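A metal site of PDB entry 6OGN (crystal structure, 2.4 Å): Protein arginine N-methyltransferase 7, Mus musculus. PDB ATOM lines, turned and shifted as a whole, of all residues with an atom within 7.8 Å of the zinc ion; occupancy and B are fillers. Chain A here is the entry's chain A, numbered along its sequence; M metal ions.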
ATOM      1  N   ASN A 194      27.483  21.216  11.592  1.00  0.00           N
ATOM      2  CA  ASN A 194      27.047  20.092  10.696  1.00  0.00           C
ATOM      3  C   ASN A 194      28.211  19.135  10.406  1.00  0.00           C
ATOM      4  O   ASN A 194      27.944  17.992  10.014  1.00  0.00           O
ATOM      5  CB  ASN A 194      26.465  20.641   9.399  1.00  0.00           C
ATOM      6  CG  ASN A 194      26.140  19.573   8.383  1.00  0.00           C
ATOM      7  OD1 ASN A 194      25.459  18.593   8.699  1.00  0.00           O
ATOM      8  ND2 ASN A 194      26.562  19.774   7.145  1.00  0.00           N
ATOM      9  N   LYS A 195      29.448  19.562  10.597  1.00  0.00           N
ATOM     10  CA  LYS A 195      30.671  18.770  10.304  1.00  0.00           C
ATOM     11  C   LYS A 195      31.628  18.826  11.486  1.00  0.00           C
ATOM     12  O   LYS A 195      31.728  19.899  12.157  1.00  0.00           O
ATOM     13  CB  LYS A 195      31.368  19.290   9.037  1.00  0.00           C
ATOM     14  CG  LYS A 195      30.612  19.074   7.741  1.00  0.00           C
ATOM     15  CD  LYS A 195      30.411  17.615   7.365  1.00  0.00           C
ATOM     16  CE  LYS A 195      29.846  17.420   5.971  1.00  0.00           C
ATOM     17  NZ  LYS A 195      28.957  16.241   5.892  1.00  0.00           N
ATOM     18  N   GLU A 215      33.026   9.019   7.021  1.00  0.00           N
ATOM     19  CA  GLU A 215      31.542   8.869   6.865  1.00  0.00           C
ATOM     20  C   GLU A 215      30.821  10.133   7.377  1.00  0.00           C
ATOM     21  O   GLU A 215      29.759  10.466   6.809  1.00  0.00           O
ATOM     22  CB  GLU A 215      31.024   7.585   7.518  1.00  0.00           C
ATOM     23  CG  GLU A 215      31.264   7.499   9.012  1.00  0.00           C
ATOM     24  CD  GLU A 215      32.540   6.783   9.403  1.00  0.00           C
ATOM     25  OE1 GLU A 215      33.528   6.805   8.593  1.00  0.00           O
ATOM     26  OE2 GLU A 215      32.552   6.195  10.495  1.00  0.00           O
ATOM     27  N   LEU A 216      31.403  10.884   8.319  1.00  0.00           N
ATOM     28  CA  LEU A 216      30.825  12.190   8.747  1.00  0.00           C
ATOM     29  C   LEU A 216      30.839  13.147   7.560  1.00  0.00           C
ATOM     30  O   LEU A 216      29.778  13.686   7.221  1.00  0.00           O
ATOM     31  CB  LEU A 216      31.587  12.787   9.928  1.00  0.00           C
ATOM     32  CG  LEU A 216      31.121  12.320  11.299  1.00  0.00           C
ATOM     33  CD1 LEU A 216      31.542  10.873  11.544  1.00  0.00           C
ATOM     34  CD2 LEU A 216      31.637  13.251  12.404  1.00  0.00           C
ATOM     35  N   GLU A 217      32.018  13.338   6.990  1.00  0.00           N
ATOM     36  CA  GLU A 217      32.254  14.221   5.823  1.00  0.00           C
ATOM     37  C   GLU A 217      31.182  13.926   4.744  1.00  0.00           C
ATOM     38  O   GLU A 217      30.655  14.891   4.182  1.00  0.00           O
ATOM     39  CB  GLU A 217      33.718  14.080   5.397  1.00  0.00           C
ATOM     40  CG  GLU A 217      33.989  14.424   3.937  1.00  0.00           C
ATOM     41  CD  GLU A 217      33.571  15.810   3.515  1.00  0.00           C
ATOM     42  OE1 GLU A 217      33.335  16.008   2.300  1.00  0.00           O
ATOM     43  OE2 GLU A 217      33.468  16.696   4.402  1.00  0.00           O
ATOM     44  N   ARG A 218      30.808  12.666   4.553  1.00  0.00           N
ATOM     45  CA  ARG A 218      29.870  12.214   3.478  1.00  0.00           C
ATOM     46  C   ARG A 218      28.391  12.327   3.925  1.00  0.00           C
ATOM     47  O   ARG A 218      27.536  12.267   3.046  1.00  0.00           O
ATOM     48  CB  ARG A 218      30.140  10.751   3.073  1.00  0.00           C
ATOM     49  CG  ARG A 218      31.470  10.512   2.358  1.00  0.00           C
ATOM     50  CD  ARG A 218      31.643   9.065   1.865  1.00  0.00           C
ATOM     51  NE  ARG A 218      32.570   8.261   2.666  1.00  0.00           N
ATOM     52  CZ  ARG A 218      32.245   7.233   3.463  1.00  0.00           C
ATOM     53  NH1 ARG A 218      33.191   6.597   4.140  1.00  0.00           N
ATOM     54  NH2 ARG A 218      30.977   6.848   3.609  1.00  0.00           N
ATOM     55  N   CYS A 219      28.088  12.379   5.225  1.00  0.00           N
ATOM     56  CA  CYS A 219      26.670  12.332   5.732  1.00  0.00           C
ATOM     57  C   CYS A 219      25.940  13.579   5.249  1.00  0.00           C
ATOM     58  O   CYS A 219      26.491  14.661   5.252  1.00  0.00           O
ATOM     59  CB  CYS A 219      26.613  12.234   7.256  1.00  0.00           C
ATOM     60  SG  CYS A 219      24.934  11.875   7.899  1.00  0.00           S
ATOM     61  N   PRO A 220      24.676  13.478   4.806  1.00  0.00           N
ATOM     62  CA  PRO A 220      23.818  14.657   4.621  1.00  0.00           C
ATOM     63  C   PRO A 220      23.487  15.438   5.897  1.00  0.00           C
ATOM     64  O   PRO A 220      22.929  16.501   5.782  1.00  0.00           O
ATOM     65  CB  PRO A 220      22.495  14.117   4.062  1.00  0.00           C
ATOM     66  CG  PRO A 220      22.564  12.593   4.271  1.00  0.00           C
ATOM     67  CD  PRO A 220      24.040  12.239   4.314  1.00  0.00           C
ATOM     68  N   GLY A 221      23.759  14.871   7.067  1.00  0.00           N
ATOM     69  CA  GLY A 221      23.431  15.492   8.362  1.00  0.00           C
ATOM     70  C   GLY A 221      22.018  15.166   8.821  1.00  0.00           C
ATOM     71  O   GLY A 221      21.298  14.416   8.091  1.00  0.00           O
ATOM     72  N   ALA A 222      21.645  15.706   9.988  1.00  0.00           N
ATOM     73  CA  ALA A 222      20.364  15.448  10.685  1.00  0.00           C
ATOM     74  C   ALA A 222      19.234  15.976   9.822  1.00  0.00           C
ATOM     75  O   ALA A 222      19.302  17.097   9.342  1.00  0.00           O
ATOM     76  CB  ALA A 222      20.392  16.116  12.059  1.00  0.00           C
ATOM     77  N   VAL A 365      18.970  10.893   5.429  1.00  0.00           N
ATOM     78  CA  VAL A 365      19.025  10.638   6.896  1.00  0.00           C
ATOM     79  C   VAL A 365      20.503  10.516   7.284  1.00  0.00           C
ATOM     80  O   VAL A 365      21.354  10.287   6.387  1.00  0.00           O
ATOM     81  CB  VAL A 365      18.253   9.352   7.264  1.00  0.00           C
ATOM     82  CG1 VAL A 365      16.877   9.308   6.597  1.00  0.00           C
ATOM     83  CG2 VAL A 365      19.052   8.094   6.909  1.00  0.00           C
ATOM     84  N   CYS A 366      20.791  10.631   8.569  1.00  0.00           N
ATOM     85  CA  CYS A 366      22.156  10.432   9.115  1.00  0.00           C
ATOM     86  C   CYS A 366      22.541   8.956   8.976  1.00  0.00           C
ATOM     87  O   CYS A 366      21.822   8.095   9.515  1.00  0.00           O
ATOM     88  CB  CYS A 366      22.222  10.881  10.563  1.00  0.00           C
ATOM     89  SG  CYS A 366      23.851  10.659  11.294  1.00  0.00           S
ATOM     90  N   ASP A 367      23.643   8.689   8.273  1.00  0.00           N
ATOM     91  CA  ASP A 367      24.256   7.338   8.146  1.00  0.00           C
ATOM     92  C   ASP A 367      25.642   7.353   8.815  1.00  0.00           C
ATOM     93  O   ASP A 367      26.448   6.459   8.508  1.00  0.00           O
ATOM     94  CB  ASP A 367      24.319   6.916   6.675  1.00  0.00           C
ATOM     95  CG  ASP A 367      25.097   7.881   5.779  1.00  0.00           C
ATOM     96  OD1 ASP A 367      25.854   8.721   6.323  1.00  0.00           O
ATOM     97  OD2 ASP A 367      24.921   7.803   4.537  1.00  0.00           O
ATOM     98  N   CYS A 368      25.935   8.340   9.668  1.00  0.00           N
ATOM     99  CA  CYS A 368      27.281   8.481  10.305  1.00  0.00           C
ATOM    100  C   CYS A 368      27.191   8.422  11.821  1.00  0.00           C
ATOM    101  O   CYS A 368      28.259   8.465  12.425  1.00  0.00           O
ATOM    102  CB  CYS A 368      28.000   9.766   9.865  1.00  0.00           C
ATOM    103  SG  CYS A 368      27.457  11.261  10.748  1.00  0.00           S
ATOM    104  N   GLN A 369      25.984   8.388  12.406  1.00  0.00           N
ATOM    105  CA  GLN A 369      25.742   8.324  13.889  1.00  0.00           C
ATOM    106  C   GLN A 369      25.881   9.713  14.563  1.00  0.00           C
ATOM    107  O   GLN A 369      25.057  10.019  15.460  1.00  0.00           O
ATOM    108  CB  GLN A 369      26.723   7.378  14.579  1.00  0.00           C
ATOM    109  CG  GLN A 369      26.897   6.016  13.902  1.00  0.00           C
ATOM    110  CD  GLN A 369      27.744   5.129  14.783  1.00  0.00           C
ATOM    111  OE1 GLN A 369      27.344   4.811  15.913  1.00  0.00           O
ATOM    112  NE2 GLN A 369      28.950   4.803  14.311  1.00  0.00           N
ATOM    113  N   ALA A 370      26.875  10.523  14.158  1.00  0.00           N
ATOM    114  CA  ALA A 370      27.311  11.755  14.861  1.00  0.00           C
ATOM    115  C   ALA A 370      26.123  12.696  15.027  1.00  0.00           C
ATOM    116  O   ALA A 370      25.961  13.245  16.116  1.00  0.00           O
ATOM    117  CB  ALA A 370      28.430  12.444  14.123  1.00  0.00           C
ATOM    118  N   HIS A 371      25.373  12.899  13.940  1.00  0.00           N
ATOM    119  CA  HIS A 371      24.263  13.875  13.831  1.00  0.00           C
ATOM    120  C   HIS A 371      23.112  13.494  14.782  1.00  0.00           C
ATOM    121  O   HIS A 371      22.334  14.403  15.132  1.00  0.00           O
ATOM    122  CB  HIS A 371      23.811  14.014  12.372  1.00  0.00           C
ATOM    123  CG  HIS A 371      24.886  14.610  11.518  1.00  0.00           C
ATOM    124  ND1 HIS A 371      25.673  13.839  10.676  1.00  0.00           N
ATOM    125  CD2 HIS A 371      25.355  15.874  11.441  1.00  0.00           C
ATOM    126  CE1 HIS A 371      26.572  14.622  10.099  1.00  0.00           C
ATOM    127  NE2 HIS A 371      26.394  15.871  10.549  1.00  0.00           N
ATOM    128  N   LEU A 372      23.020  12.228  15.200  1.00  0.00           N
ATOM    129  CA  LEU A 372      21.953  11.735  16.111  1.00  0.00           C
ATOM    130  C   LEU A 372      22.366  11.908  17.586  1.00  0.00           C
ATOM    131  O   LEU A 372      21.456  11.912  18.426  1.00  0.00           O
ATOM    132  CB  LEU A 372      21.651  10.255  15.799  1.00  0.00           C
ATOM    133  CG  LEU A 372      21.083   9.978  14.398  1.00  0.00           C
ATOM    134  CD1 LEU A 372      20.792   8.490  14.218  1.00  0.00           C
ATOM    135  CD2 LEU A 372      19.835  10.809  14.112  1.00  0.00           C
ATOM    136  N   PHE A 379      28.174  20.352  18.094  1.00  0.00           N
ATOM    137  CA  PHE A 379      29.123  20.362  16.954  1.00  0.00           C
ATOM    138  C   PHE A 379      29.937  21.647  17.015  1.00  0.00           C
ATOM    139  O   PHE A 379      31.169  21.567  17.012  1.00  0.00           O
ATOM    140  CB  PHE A 379      28.374  20.260  15.614  1.00  0.00           C
ATOM    141  CG  PHE A 379      28.319  18.868  15.051  1.00  0.00           C
ATOM    142  CD1 PHE A 379      29.333  18.397  14.229  1.00  0.00           C
ATOM    143  CD2 PHE A 379      27.201  18.051  15.272  1.00  0.00           C
ATOM    144  CE1 PHE A 379      29.230  17.151  13.632  1.00  0.00           C
ATOM    145  CE2 PHE A 379      27.124  16.791  14.704  1.00  0.00           C
ATOM    146  CZ  PHE A 379      28.149  16.342  13.888  1.00  0.00           C
HETATM  147 ZN    ZN M   1      25.463  11.882  10.070  1.00  0.00          ZN
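A ring nitrogen (NE2) of His 371 sits at hydrogen-bond distance from the backbone carbonyl oxygen of Asn 194.
The side-chain sulfur of Cys 368 sits close to the backbone NH of Ala 370 (3.5 Å).
The side-chain sulfur (SG) of Cys 219 lies close to the backbone NH (N) of Asp 367 (3.5 Å).
The side-chain sulfur (SG) of Cys 219 sits close to the backbone NH (N) of Gly 221.
NZ of Lys 195 is in hydrogen-bond range of O of Cys 219 (3.0 Å).
N of Gln 369 lies close to SG of Cys 366, 3.3 Å away.
Of the 19 residues printed, 4 come within 4 Å of the zinc ion.
A ring nitrogen (ND1) of His 371 binds the zinc ion, 2.1 Å away.
SG of Cys 368 binds the zinc ion (2.2 Å).
The zinc ion is bound by SG of Cys 219 (2.2 Å).
SG of Cys 366 is bound to the zinc ion (2.4 Å).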
